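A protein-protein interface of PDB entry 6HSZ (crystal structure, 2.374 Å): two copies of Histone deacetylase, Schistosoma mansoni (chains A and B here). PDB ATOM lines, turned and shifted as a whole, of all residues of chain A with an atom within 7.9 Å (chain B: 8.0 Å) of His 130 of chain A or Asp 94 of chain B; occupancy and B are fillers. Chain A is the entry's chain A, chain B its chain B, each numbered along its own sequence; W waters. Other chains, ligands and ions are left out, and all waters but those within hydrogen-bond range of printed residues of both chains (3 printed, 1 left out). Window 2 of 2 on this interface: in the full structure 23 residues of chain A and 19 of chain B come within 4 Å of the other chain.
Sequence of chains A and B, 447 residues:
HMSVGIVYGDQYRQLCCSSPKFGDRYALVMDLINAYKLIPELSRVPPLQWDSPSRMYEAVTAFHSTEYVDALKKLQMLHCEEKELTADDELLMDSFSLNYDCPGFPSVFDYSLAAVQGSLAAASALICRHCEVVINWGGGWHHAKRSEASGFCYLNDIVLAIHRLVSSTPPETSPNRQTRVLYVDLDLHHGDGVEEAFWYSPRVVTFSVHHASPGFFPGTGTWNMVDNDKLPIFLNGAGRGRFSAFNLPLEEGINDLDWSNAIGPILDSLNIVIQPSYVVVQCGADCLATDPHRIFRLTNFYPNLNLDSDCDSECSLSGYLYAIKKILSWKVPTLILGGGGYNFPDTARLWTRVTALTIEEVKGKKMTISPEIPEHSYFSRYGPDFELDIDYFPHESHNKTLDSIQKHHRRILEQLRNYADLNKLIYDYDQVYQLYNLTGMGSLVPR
NH2 of Arg 44 of chain A lies within hydrogen-bond range of OG of Ser 97 of chain B (2.8 Å).
The guanidinium group (NH2) of Arg 44 of chain A lies within salt-bridge range of the side-chain carboxylate (OE2) of Glu 148 of chain B (3.5 Å).
The side-chain carboxylate of Asp 94 of chain B lies within hydrogen-bond range of a ring nitrogen (NE2) of His 130 of chain A, 3.1 Å away.
OD2 of Asp 94 of chain B is in hydrogen-bond range of OG of Ser 43 of chain A (3.0 Å).
The backbone carbonyl oxygen (O) of Ser 97 of chain B sits close to the side-chain amide oxygen (OD1) of Asn 99 of chain B, at 3.4 Å.
Among the printed residues, merely in contact across the chains: Leu 42 of chain A with Leu 91 of chain B (3.6 Å), Ser 43 of chain A with Leu 91 of chain B (3.6 Å), Val 45 of chain A with Tyr 100 of chain B (3.7 Å), Pro 46 of chain A with Tyr 100 of chain B (3.5 Å), Ala 125 of chain A with Tyr 100 of chain B (3.9 Å) and His 130 of chain A with Tyr 100 of chain B (3.4 Å).
Val 4 of chain A touches none of the printed residues of chain B.
Of the printed residues of chain B, Arg 44 of chain A touches Ser 97 (2.8 Å) and Glu 148 (3.5 Å).
Of the printed residues of chain B, Ala 125 of chain A touches Tyr 100.
Of chain B, only Asp 94 (3.1 Å) and Tyr 100 (3.4 Å) come within 4 Å of His 130 of chain A.
Of chain A, only Ser 43 (3.0 Å) and His 130 (3.1 Å) come within 4 Å of Asp 94 of chain B.
The nearest residue of chain B that does not touch His 130 of chain A is Glu 90 of chain B (4.3 Å).
The nearest residue of chain A that does not touch Asp 94 of chain B is Arg 44 of chain A (4.3 Å).
Of the 19 printed residues of chain B, 5 touch a printed residue of chain A.
Printed residues of chain B that touch a printed residue of chain A: Leu 91, Asp 94, Ser 97, Tyr 100 and Glu 148.
Of the 20 printed residues of chain A, 7 touch a printed residue of chain B.
Hydrophobic or aromatic side chains of chain A within 4 Å of the printed part of chain B: Val 45, Pro 46, Ala 125 and His 130.
Among the printed residues, Asp or Glu carboxylates within 4 Å of a Lys or Arg side-chain nitrogen of the other chain: Arg 44 of chain A with Glu 148 of chain B.
No position is printed for both chains.
Of the 10 pairs that touch across the chains among the printed residues, none has its exchanged pair printed and touching as well.
Water W1 lies within hydrogen-bond range of the guanidinium group (NE) of Arg 44 of chain A, the side-chain hydroxyl (OG) of Ser 97 of chain B, the backbone carbonyl oxygen (O) of Asp 94 of chain B and the backbone carbonyl oxygen (O) of Ser 95 of chain B.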
ATOM      1  N   SER A   3     -13.699   6.859  -1.929  1.00  0.00           N
ATOM      2  CA  SER A   3     -13.245   5.542  -2.350  1.00  0.00           C
ATOM      3  C   SER A   3     -14.434   4.716  -2.865  1.00  0.00           C
ATOM      4  O   SER A   3     -15.558   5.213  -2.925  1.00  0.00           O
ATOM      5  CB  SER A   3     -12.546   4.826  -1.193  1.00  0.00           C
ATOM      6  OG  SER A   3     -13.483   4.214  -0.319  1.00  0.00           O
ATOM      7  N   VAL A   4     -14.170   3.468  -3.253  1.00  0.00           N
ATOM      8  CA  VAL A   4     -15.190   2.537  -3.732  1.00  0.00           C
ATOM      9  C   VAL A   4     -15.170   1.321  -2.819  1.00  0.00           C
ATOM     10  O   VAL A   4     -14.122   0.675  -2.665  1.00  0.00           O
ATOM     11  CB  VAL A   4     -14.952   2.108  -5.187  1.00  0.00           C
ATOM     12  CG1 VAL A   4     -16.026   1.097  -5.598  1.00  0.00           C
ATOM     13  CG2 VAL A   4     -14.939   3.301  -6.117  1.00  0.00           C
ATOM     14  N   GLY A   5     -16.321   0.998  -2.234  1.00  0.00           N
ATOM     15  CA  GLY A   5     -16.429  -0.075  -1.259  1.00  0.00           C
ATOM     16  C   GLY A   5     -17.147  -1.278  -1.844  1.00  0.00           C
ATOM     17  O   GLY A   5     -18.030  -1.138  -2.691  1.00  0.00           O
ATOM     18  N   TYR A   8     -18.033  -7.764   1.427  1.00  0.00           N
ATOM     19  CA  TYR A   8     -17.781  -9.201   1.425  1.00  0.00           C
ATOM     20  C   TYR A   8     -17.238  -9.619   2.780  1.00  0.00           C
ATOM     21  O   TYR A   8     -17.040  -8.806   3.683  1.00  0.00           O
ATOM     22  CB  TYR A   8     -16.844  -9.648   0.293  1.00  0.00           C
ATOM     23  CG  TYR A   8     -15.405  -9.212   0.377  1.00  0.00           C
ATOM     24  CD1 TYR A   8     -14.988  -8.027  -0.228  1.00  0.00           C
ATOM     25  CD2 TYR A   8     -14.440 -10.002   1.011  1.00  0.00           C
ATOM     26  CE1 TYR A   8     -13.651  -7.606  -0.173  1.00  0.00           C
ATOM     27  CE2 TYR A   8     -13.084  -9.593   1.068  1.00  0.00           C
ATOM     28  CZ  TYR A   8     -12.703  -8.389   0.473  1.00  0.00           C
ATOM     29  OH  TYR A   8     -11.387  -7.956   0.511  1.00  0.00           O
ATOM     30  N   LEU A  42     -10.378  -1.877  -4.123  1.00  0.00           N
ATOM     31  CA  LEU A  42     -11.650  -1.671  -3.444  1.00  0.00           C
ATOM     32  C   LEU A  42     -11.494  -1.711  -1.924  1.00  0.00           C
ATOM     33  O   LEU A  42     -10.665  -2.444  -1.380  1.00  0.00           O
ATOM     34  CB  LEU A  42     -12.665  -2.732  -3.887  1.00  0.00           C
ATOM     35  CG  LEU A  42     -12.943  -2.809  -5.390  1.00  0.00           C
ATOM     36  CD1 LEU A  42     -13.599  -4.125  -5.789  1.00  0.00           C
ATOM     37  CD2 LEU A  42     -13.839  -1.668  -5.749  1.00  0.00           C
ATOM     38  N   SER A  43     -12.314  -0.929  -1.237  1.00  0.00           N
ATOM     39  CA  SER A  43     -12.349  -0.928   0.222  1.00  0.00           C
ATOM     40  C   SER A  43     -13.379  -1.953   0.697  1.00  0.00           C
ATOM     41  O   SER A  43     -14.552  -1.867   0.323  1.00  0.00           O
ATOM     42  CB  SER A  43     -12.691   0.477   0.714  1.00  0.00           C
ATOM     43  OG  SER A  43     -13.238   0.466   2.017  1.00  0.00           O
ATOM     44  N   ARG A  44     -12.955  -2.929   1.507  1.00  0.00           N
ATOM     45  CA  ARG A  44     -13.894  -3.965   1.947  1.00  0.00           C
ATOM     46  C   ARG A  44     -14.815  -3.420   3.033  1.00  0.00           C
ATOM     47  O   ARG A  44     -14.339  -2.975   4.078  1.00  0.00           O
ATOM     48  CB  ARG A  44     -13.203  -5.212   2.488  1.00  0.00           C
ATOM     49  CG  ARG A  44     -14.254  -6.115   3.180  1.00  0.00           C
ATOM     50  CD  ARG A  44     -13.743  -7.472   3.615  1.00  0.00           C
ATOM     51  NE  ARG A  44     -13.188  -7.469   4.965  1.00  0.00           N
ATOM     52  CZ  ARG A  44     -13.833  -7.867   6.059  1.00  0.00           C
ATOM     53  NH1 ARG A  44     -15.089  -8.320   6.008  1.00  0.00           N
ATOM     54  NH2 ARG A  44     -13.208  -7.814   7.220  1.00  0.00           N
ATOM     55  N   VAL A  45     -16.124  -3.492   2.802  1.00  0.00           N
ATOM     56  CA  VAL A  45     -17.130  -3.082   3.778  1.00  0.00           C
ATOM     57  C   VAL A  45     -17.666  -4.337   4.472  1.00  0.00           C
ATOM     58  O   VAL A  45     -18.368  -5.130   3.825  1.00  0.00           O
ATOM     59  CB  VAL A  45     -18.262  -2.297   3.108  1.00  0.00           C
ATOM     60  CG1 VAL A  45     -19.383  -2.012   4.117  1.00  0.00           C
ATOM     61  CG2 VAL A  45     -17.725  -1.015   2.516  1.00  0.00           C
ATOM     62  N   PRO A  46     -17.405  -4.533   5.776  1.00  0.00           N
ATOM     63  CA  PRO A  46     -17.882  -5.747   6.441  1.00  0.00           C
ATOM     64  C   PRO A  46     -19.374  -5.658   6.694  1.00  0.00           C
ATOM     65  O   PRO A  46     -19.914  -4.564   6.943  1.00  0.00           O
ATOM     66  CB  PRO A  46     -17.104  -5.751   7.766  1.00  0.00           C
ATOM     67  CG  PRO A  46     -16.994  -4.271   8.064  1.00  0.00           C
ATOM     68  CD  PRO A  46     -16.789  -3.600   6.737  1.00  0.00           C
ATOM     69  N   SER A 124     -24.258   2.782   5.626  1.00  0.00           N
ATOM     70  CA  SER A 124     -23.507   3.479   6.661  1.00  0.00           C
ATOM     71  C   SER A 124     -22.156   3.957   6.149  1.00  0.00           C
ATOM     72  O   SER A 124     -21.700   5.050   6.507  1.00  0.00           O
ATOM     73  CB  SER A 124     -23.334   2.571   7.878  1.00  0.00           C
ATOM     74  OG  SER A 124     -24.560   2.483   8.579  1.00  0.00           O
ATOM     75  N   ALA A 125     -21.500   3.158   5.310  1.00  0.00           N
ATOM     76  CA  ALA A 125     -20.228   3.604   4.748  1.00  0.00           C
ATOM     77  C   ALA A 125     -20.420   4.848   3.885  1.00  0.00           C
ATOM     78  O   ALA A 125     -19.540   5.715   3.840  1.00  0.00           O
ATOM     79  CB  ALA A 125     -19.578   2.471   3.957  1.00  0.00           C
ATOM     80  N   LEU A 126     -21.560   4.953   3.191  1.00  0.00           N
ATOM     81  CA  LEU A 126     -21.862   6.182   2.455  1.00  0.00           C
ATOM     82  C   LEU A 126     -22.125   7.347   3.398  1.00  0.00           C
ATOM     83  O   LEU A 126     -21.719   8.479   3.120  1.00  0.00           O
ATOM     84  CB  LEU A 126     -23.075   5.979   1.539  1.00  0.00           C
ATOM     85  CG  LEU A 126     -22.878   5.097   0.315  1.00  0.00           C
ATOM     86  CD1 LEU A 126     -24.130   5.084  -0.550  1.00  0.00           C
ATOM     87  CD2 LEU A 126     -21.704   5.616  -0.479  1.00  0.00           C
ATOM     88  N   ILE A 127     -22.806   7.092   4.515  1.00  0.00           N
ATOM     89  CA  ILE A 127     -23.300   8.185   5.347  1.00  0.00           C
ATOM     90  C   ILE A 127     -22.152   8.847   6.095  1.00  0.00           C
ATOM     91  O   ILE A 127     -22.040  10.077   6.123  1.00  0.00           O
ATOM     92  CB  ILE A 127     -24.382   7.675   6.305  1.00  0.00           C
ATOM     93  CG1 ILE A 127     -25.646   7.324   5.529  1.00  0.00           C
ATOM     94  CG2 ILE A 127     -24.676   8.695   7.371  1.00  0.00           C
ATOM     95  CD1 ILE A 127     -26.573   6.383   6.306  1.00  0.00           C
ATOM     96  N   CYS A 128     -21.289   8.050   6.728  1.00  0.00           N
ATOM     97  CA  CYS A 128     -20.109   8.588   7.389  1.00  0.00           C
ATOM     98  C   CYS A 128     -19.089   9.136   6.397  1.00  0.00           C
ATOM     99  O   CYS A 128     -18.111   9.756   6.822  1.00  0.00           O
ATOM    100  CB  CYS A 128     -19.455   7.514   8.262  1.00  0.00           C
ATOM    101  SG  CYS A 128     -18.642   6.156   7.354  1.00  0.00           S
ATOM    102  N   ARG A 129     -19.287   8.893   5.094  1.00  0.00           N
ATOM    103  CA  ARG A 129     -18.463   9.376   3.982  1.00  0.00           C
ATOM    104  C   ARG A 129     -17.128   8.641   3.850  1.00  0.00           C
ATOM    105  O   ARG A 129     -16.182   9.176   3.264  1.00  0.00           O
ATOM    106  CB  ARG A 129     -18.232  10.895   4.067  1.00  0.00           C
ATOM    107  CG  ARG A 129     -19.499  11.753   3.879  1.00  0.00           C
ATOM    108  CD  ARG A 129     -20.237  11.407   2.574  1.00  0.00           C
ATOM    109  NE  ARG A 129     -21.287  12.368   2.198  1.00  0.00           N
ATOM    110  CZ  ARG A 129     -22.605  12.193   2.359  1.00  0.00           C
ATOM    111  NH1 ARG A 129     -23.092  11.081   2.905  1.00  0.00           N
ATOM    112  NH2 ARG A 129     -23.445  13.148   1.968  1.00  0.00           N
ATOM    113  N   HIS A 130     -17.039   7.406   4.356  1.00  0.00           N
ATOM    114  CA  HIS A 130     -15.859   6.571   4.140  1.00  0.00           C
ATOM    115  C   HIS A 130     -15.723   6.148   2.677  1.00  0.00           C
ATOM    116  O   HIS A 130     -14.603   5.992   2.172  1.00  0.00           O
ATOM    117  CB  HIS A 130     -15.933   5.340   5.052  1.00  0.00           C
ATOM    118  CG  HIS A 130     -14.694   4.491   5.057  1.00  0.00           C
ATOM    119  ND1 HIS A 130     -13.553   4.838   5.756  1.00  0.00           N
ATOM    120  CD2 HIS A 130     -14.425   3.304   4.460  1.00  0.00           C
ATOM    121  CE1 HIS A 130     -12.634   3.903   5.584  1.00  0.00           C
ATOM    122  NE2 HIS A 130     -13.138   2.961   4.804  1.00  0.00           N
ATOM    123  N   CYS A 131     -16.843   5.936   1.995  1.00  0.00           N
ATOM    124  CA  CYS A 131     -16.852   5.547   0.595  1.00  0.00           C
ATOM    125  C   CYS A 131     -17.765   6.495  -0.161  1.00  0.00           C
ATOM    126  O   CYS A 131     -18.757   6.996   0.382  1.00  0.00           O
ATOM    127  CB  CYS A 131     -17.333   4.100   0.398  1.00  0.00           C
ATOM    128  SG  CYS A 131     -16.427   2.825   1.323  1.00  0.00           S
ATOM    129  N   GLU A 132     -17.405   6.755  -1.411  1.00  0.00           N
ATOM    130  CA  GLU A 132     -18.261   7.512  -2.314  1.00  0.00           C
ATOM    131  C   GLU A 132     -19.267   6.600  -3.000  1.00  0.00           C
ATOM    132  O   GLU A 132     -20.420   6.991  -3.211  1.00  0.00           O
ATOM    133  CB  GLU A 132     -17.397   8.242  -3.352  1.00  0.00           C
ATOM    134  CG  GLU A 132     -16.234   8.996  -2.720  1.00  0.00           C
ATOM    135  CD  GLU A 132     -15.279   9.593  -3.739  1.00  0.00           C
ATOM    136  OE1 GLU A 132     -15.335   9.196  -4.923  1.00  0.00           O
ATOM    137  OE2 GLU A 132     -14.476  10.473  -3.351  1.00  0.00           O
ATOM    138  N   VAL A 133     -18.838   5.384  -3.329  1.00  0.00           N
ATOM    139  CA  VAL A 133     -19.674   4.334  -3.883  1.00  0.00           C
ATOM    140  C   VAL A 133     -19.428   3.069  -3.062  1.00  0.00           C
ATOM    141  O   VAL A 133     -18.303   2.843  -2.584  1.00  0.00           O
ATOM    142  CB  VAL A 133     -19.363   4.113  -5.387  1.00  0.00           C
ATOM    143  CG1 VAL A 133     -20.192   2.943  -5.970  1.00  0.00           C
ATOM    144  CG2 VAL A 133     -19.647   5.401  -6.169  1.00  0.00           C
ATOM    145  N   VAL A 134     -20.491   2.275  -2.846  1.00  0.00           N
ATOM    146  CA  VAL A 134     -20.399   0.941  -2.247  1.00  0.00           C
ATOM    147  C   VAL A 134     -21.189  -0.048  -3.091  1.00  0.00           C
ATOM    148  O   VAL A 134     -22.322   0.234  -3.499  1.00  0.00           O
ATOM    149  CB  VAL A 134     -20.924   0.868  -0.798  1.00  0.00           C
ATOM    150  CG1 VAL A 134     -20.558  -0.491  -0.214  1.00  0.00           C
ATOM    151  CG2 VAL A 134     -20.378   1.983   0.044  1.00  0.00           C
ATOM    152  N   ALA B  71       1.235  -2.965   9.163  1.00  0.00           N
ATOM    153  CA  ALA B  71       0.112  -2.051   8.997  1.00  0.00           C
ATOM    154  C   ALA B  71      -0.354  -1.499  10.332  1.00  0.00           C
ATOM    155  O   ALA B  71      -0.780  -0.347  10.408  1.00  0.00           O
ATOM    156  CB  ALA B  71      -1.046  -2.762   8.300  1.00  0.00           C
ATOM    157  N   LEU B  75      -0.559   2.433  11.333  1.00  0.00           N
ATOM    158  CA  LEU B  75      -1.802   3.087  11.715  1.00  0.00           C
ATOM    159  C   LEU B  75      -1.592   3.957  12.951  1.00  0.00           C
ATOM    160  O   LEU B  75      -2.145   5.060  13.052  1.00  0.00           O
ATOM    161  CB  LEU B  75      -2.886   2.030  11.953  1.00  0.00           C
ATOM    162  CG  LEU B  75      -4.306   2.429  12.378  1.00  0.00           C
ATOM    163  CD1 LEU B  75      -4.951   3.356  11.373  1.00  0.00           C
ATOM    164  CD2 LEU B  75      -5.176   1.173  12.573  1.00  0.00           C
ATOM    165  N   LEU B  85      -4.878  10.656   6.333  1.00  0.00           N
ATOM    166  CA  LEU B  85      -4.596   9.401   5.629  1.00  0.00           C
ATOM    167  C   LEU B  85      -4.691   9.571   4.115  1.00  0.00           C
ATOM    168  O   LEU B  85      -5.595  10.252   3.628  1.00  0.00           O
ATOM    169  CB  LEU B  85      -5.559   8.294   6.077  1.00  0.00           C
ATOM    170  CG  LEU B  85      -5.012   7.190   6.986  1.00  0.00           C
ATOM    171  CD1 LEU B  85      -5.007   7.633   8.444  1.00  0.00           C
ATOM    172  CD2 LEU B  85      -5.770   5.875   6.810  1.00  0.00           C
ATOM    173  N   ALA B  87      -5.322   7.940   0.233  1.00  0.00           N
ATOM    174  CA  ALA B  87      -6.306   6.973  -0.243  1.00  0.00           C
ATOM    175  C   ALA B  87      -5.753   5.550  -0.248  1.00  0.00           C
ATOM    176  O   ALA B  87      -6.510   4.593  -0.064  1.00  0.00           O
ATOM    177  CB  ALA B  87      -6.800   7.366  -1.635  1.00  0.00           C
ATOM    178  N   ASP B  88      -4.445   5.383  -0.423  1.00  0.00           N
ATOM    179  CA  ASP B  88      -3.884   4.040  -0.366  1.00  0.00           C
ATOM    180  C   ASP B  88      -3.541   3.597   1.056  1.00  0.00           C
ATOM    181  O   ASP B  88      -3.553   2.391   1.337  1.00  0.00           O
ATOM    182  CB  ASP B  88      -2.670   3.959  -1.286  1.00  0.00           C
ATOM    183  CG  ASP B  88      -3.047   4.216  -2.729  1.00  0.00           C
ATOM    184  OD1 ASP B  88      -4.027   3.588  -3.196  1.00  0.00           O
ATOM    185  OD2 ASP B  88      -2.401   5.074  -3.374  1.00  0.00           O
ATOM    186  N   ASP B  89      -3.279   4.539   1.967  1.00  0.00           N
ATOM    187  CA  ASP B  89      -3.293   4.203   3.386  1.00  0.00           C
ATOM    188  C   ASP B  89      -4.684   3.752   3.830  1.00  0.00           C
ATOM    189  O   ASP B  89      -4.811   2.776   4.579  1.00  0.00           O
ATOM    190  CB  ASP B  89      -2.814   5.396   4.206  1.00  0.00           C
ATOM    191  CG  ASP B  89      -1.364   5.726   3.932  1.00  0.00           C
ATOM    192  OD1 ASP B  89      -0.629   4.808   3.475  1.00  0.00           O
ATOM    193  OD2 ASP B  89      -0.976   6.903   4.161  1.00  0.00           O
ATOM    194  N   GLU B  90      -5.737   4.445   3.364  1.00  0.00           N
ATOM    195  CA  GLU B  90      -7.113   4.010   3.613  1.00  0.00           C
ATOM    196  C   GLU B  90      -7.364   2.593   3.097  1.00  0.00           C
ATOM    197  O   GLU B  90      -7.902   1.746   3.824  1.00  0.00           O
ATOM    198  CB  GLU B  90      -8.107   4.986   2.976  1.00  0.00           C
ATOM    199  CG  GLU B  90      -7.979   6.443   3.422  1.00  0.00           C
ATOM    200  CD  GLU B  90      -8.778   6.792   4.669  1.00  0.00           C
ATOM    201  OE1 GLU B  90      -8.887   5.955   5.591  1.00  0.00           O
ATOM    202  OE2 GLU B  90      -9.294   7.926   4.728  1.00  0.00           O
ATOM    203  N   LEU B  91      -6.989   2.310   1.839  1.00  0.00           N
ATOM    204  CA  LEU B  91      -7.193   0.955   1.311  1.00  0.00           C
ATOM    205  C   LEU B  91      -6.390  -0.071   2.107  1.00  0.00           C
ATOM    206  O   LEU B  91      -6.919  -1.118   2.500  1.00  0.00           O
ATOM    207  CB  LEU B  91      -6.825   0.879  -0.171  1.00  0.00           C
ATOM    208  CG  LEU B  91      -7.744   1.492  -1.230  1.00  0.00           C
ATOM    209  CD1 LEU B  91      -7.122   1.339  -2.612  1.00  0.00           C
ATOM    210  CD2 LEU B  91      -9.121   0.838  -1.194  1.00  0.00           C
ATOM    211  N   LEU B  92      -5.110   0.221   2.356  1.00  0.00           N
ATOM    212  CA  LEU B  92      -4.263  -0.665   3.150  1.00  0.00           C
ATOM    213  C   LEU B  92      -4.903  -1.007   4.498  1.00  0.00           C
ATOM    214  O   LEU B  92      -4.985  -2.181   4.878  1.00  0.00           O
ATOM    215  CB  LEU B  92      -2.883  -0.018   3.348  1.00  0.00           C
ATOM    216  CG  LEU B  92      -1.977  -0.665   4.416  1.00  0.00           C
ATOM    217  CD1 LEU B  92      -1.346  -1.976   3.912  1.00  0.00           C
ATOM    218  CD2 LEU B  92      -0.907   0.293   4.988  1.00  0.00           C
ATOM    219  N   MET B  93      -5.378   0.004   5.233  1.00  0.00           N
ATOM    220  CA  MET B  93      -5.975  -0.277   6.537  1.00  0.00           C
ATOM    221  C   MET B  93      -7.243  -1.129   6.409  1.00  0.00           C
ATOM    222  O   MET B  93      -7.438  -2.076   7.180  1.00  0.00           O
ATOM    223  CB  MET B  93      -6.244   1.030   7.286  1.00  0.00           C
ATOM    224  CG  MET B  93      -4.958   1.825   7.610  1.00  0.00           C
ATOM    225  SD  MET B  93      -3.668   0.875   8.490  1.00  0.00           S
ATOM    226  CE  MET B  93      -2.203   1.737   7.953  1.00  0.00           C
ATOM    227  N   ASP B  94      -8.102  -0.837   5.431  1.00  0.00           N
ATOM    228  CA  ASP B  94      -9.328  -1.628   5.285  1.00  0.00           C
ATOM    229  C   ASP B  94      -9.038  -3.078   4.898  1.00  0.00           C
ATOM    230  O   ASP B  94      -9.829  -3.974   5.219  1.00  0.00           O
ATOM    231  CB  ASP B  94     -10.273  -0.984   4.259  1.00  0.00           C
ATOM    232  CG  ASP B  94     -10.613   0.468   4.593  1.00  0.00           C
ATOM    233  OD1 ASP B  94     -10.637   0.828   5.794  1.00  0.00           O
ATOM    234  OD2 ASP B  94     -10.840   1.257   3.654  1.00  0.00           O
ATOM    235  N   SER B  95      -7.911  -3.340   4.237  1.00  0.00           N
ATOM    236  CA  SER B  95      -7.563  -4.722   3.941  1.00  0.00           C
ATOM    237  C   SER B  95      -7.275  -5.531   5.207  1.00  0.00           C
ATOM    238  O   SER B  95      -7.255  -6.764   5.139  1.00  0.00           O
ATOM    239  CB  SER B  95      -6.353  -4.764   3.000  1.00  0.00           C
ATOM    240  OG  SER B  95      -5.134  -4.774   3.723  1.00  0.00           O
ATOM    241  N   PHE B  96      -7.022  -4.869   6.343  1.00  0.00           N
ATOM    242  CA  PHE B  96      -6.773  -5.540   7.614  1.00  0.00           C
ATOM    243  C   PHE B  96      -7.900  -5.300   8.610  1.00  0.00           C
ATOM    244  O   PHE B  96      -7.744  -5.584   9.808  1.00  0.00           O
ATOM    245  CB  PHE B  96      -5.422  -5.101   8.202  1.00  0.00           C
ATOM    246  CG  PHE B  96      -4.225  -5.463   7.324  1.00  0.00           C
ATOM    247  CD1 PHE B  96      -3.772  -6.777   7.242  1.00  0.00           C
ATOM    248  CD2 PHE B  96      -3.572  -4.492   6.572  1.00  0.00           C
ATOM    249  CE1 PHE B  96      -2.681  -7.112   6.421  1.00  0.00           C
ATOM    250  CE2 PHE B  96      -2.473  -4.820   5.771  1.00  0.00           C
ATOM    251  CZ  PHE B  96      -2.031  -6.127   5.691  1.00  0.00           C
ATOM    252  N   SER B  97      -9.037  -4.786   8.137  1.00  0.00           N
ATOM    253  CA  SER B  97     -10.151  -4.412   9.002  1.00  0.00           C
ATOM    254  C   SER B  97      -9.697  -3.451  10.106  1.00  0.00           C
ATOM    255  O   SER B  97     -10.231  -3.458  11.217  1.00  0.00           O
ATOM    256  CB  SER B  97     -10.826  -5.658   9.582  1.00  0.00           C
ATOM    257  OG  SER B  97     -11.129  -6.566   8.529  1.00  0.00           O
ATOM    258  N   LEU B  98      -8.684  -2.641   9.800  1.00  0.00           N
ATOM    259  CA  LEU B  98      -8.261  -1.538  10.662  1.00  0.00           C
ATOM    260  C   LEU B  98      -9.183  -0.340  10.418  1.00  0.00           C
ATOM    261  O   LEU B  98      -8.778   0.732   9.972  1.00  0.00           O
ATOM    262  CB  LEU B  98      -6.789  -1.214  10.416  1.00  0.00           C
ATOM    263  CG  LEU B  98      -5.933  -2.382  10.931  1.00  0.00           C
ATOM    264  CD1 LEU B  98      -4.469  -2.276  10.569  1.00  0.00           C
ATOM    265  CD2 LEU B  98      -6.107  -2.565  12.458  1.00  0.00           C
ATOM    266  N   ASN B  99     -10.464  -0.561  10.703  1.00  0.00           N
ATOM    267  CA  ASN B  99     -11.513   0.412  10.421  1.00  0.00           C
ATOM    268  C   ASN B  99     -12.716   0.082  11.292  1.00  0.00           C
ATOM    269  O   ASN B  99     -12.681  -0.853  12.097  1.00  0.00           O
ATOM    270  CB  ASN B  99     -11.883   0.415   8.931  1.00  0.00           C
ATOM    271  CG  ASN B  99     -12.117  -0.993   8.376  1.00  0.00           C
ATOM    272  OD1 ASN B  99     -12.424  -1.922   9.118  1.00  0.00           O
ATOM    273  ND2 ASN B  99     -11.984  -1.144   7.064  1.00  0.00           N
ATOM    274  N   TYR B 100     -13.783   0.867  11.112  1.00  0.00           N
ATOM    275  CA  TYR B 100     -15.079   0.719  11.780  1.00  0.00           C
ATOM    276  C   TYR B 100     -14.953   0.385  13.265  1.00  0.00           C
ATOM    277  O   TYR B 100     -14.643   1.267  14.070  1.00  0.00           O
ATOM    278  CB  TYR B 100     -15.934  -0.340  11.059  1.00  0.00           C
ATOM    279  CG  TYR B 100     -16.089  -0.060   9.572  1.00  0.00           C
ATOM    280  CD1 TYR B 100     -16.987   0.895   9.108  1.00  0.00           C
ATOM    281  CD2 TYR B 100     -15.312  -0.729   8.643  1.00  0.00           C
ATOM    282  CE1 TYR B 100     -17.107   1.166   7.753  1.00  0.00           C
ATOM    283  CE2 TYR B 100     -15.420  -0.465   7.298  1.00  0.00           C
ATOM    284  CZ  TYR B 100     -16.320   0.478   6.853  1.00  0.00           C
ATOM    285  OH  TYR B 100     -16.423   0.728   5.500  1.00  0.00           O
ATOM    286  N   SER B 147      -4.247 -11.985  10.333  1.00  0.00           N
ATOM    287  CA  SER B 147      -4.040 -10.802   9.517  1.00  0.00           C
ATOM    288  C   SER B 147      -5.235  -9.863   9.586  1.00  0.00           C
ATOM    289  O   SER B 147      -5.551  -9.193   8.600  1.00  0.00           O
ATOM    290  CB  SER B 147      -3.778 -11.202   8.071  1.00  0.00           C
ATOM    291  OG  SER B 147      -2.493 -11.750   7.959  1.00  0.00           O
ATOM    292  N   GLU B 148      -5.901  -9.791  10.741  1.00  0.00           N
ATOM    293  CA  GLU B 148      -7.166  -9.070  10.783  1.00  0.00           C
ATOM    294  C   GLU B 148      -7.497  -8.637  12.209  1.00  0.00           C
ATOM    295  O   GLU B 148      -7.524  -9.468  13.123  1.00  0.00           O
ATOM    296  CB  GLU B 148      -8.286  -9.959  10.207  1.00  0.00           C
ATOM    297  CG  GLU B 148      -9.594  -9.250   9.996  1.00  0.00           C
ATOM    298  CD  GLU B 148     -10.655 -10.166   9.441  1.00  0.00           C
ATOM    299  OE1 GLU B 148     -10.292 -11.156   8.779  1.00  0.00           O
ATOM    300  OE2 GLU B 148     -11.849  -9.902   9.678  1.00  0.00           O
HETATM  301  O   HOH W   1     -10.453  -7.100   5.493  1.00  0.00           O
HETATM  302  O   HOH W   2     -10.068  -7.105   3.123  1.00  0.00           O
HETATM  303  O   HOH W   3     -10.095  -3.736   1.728  1.00  0.00           O
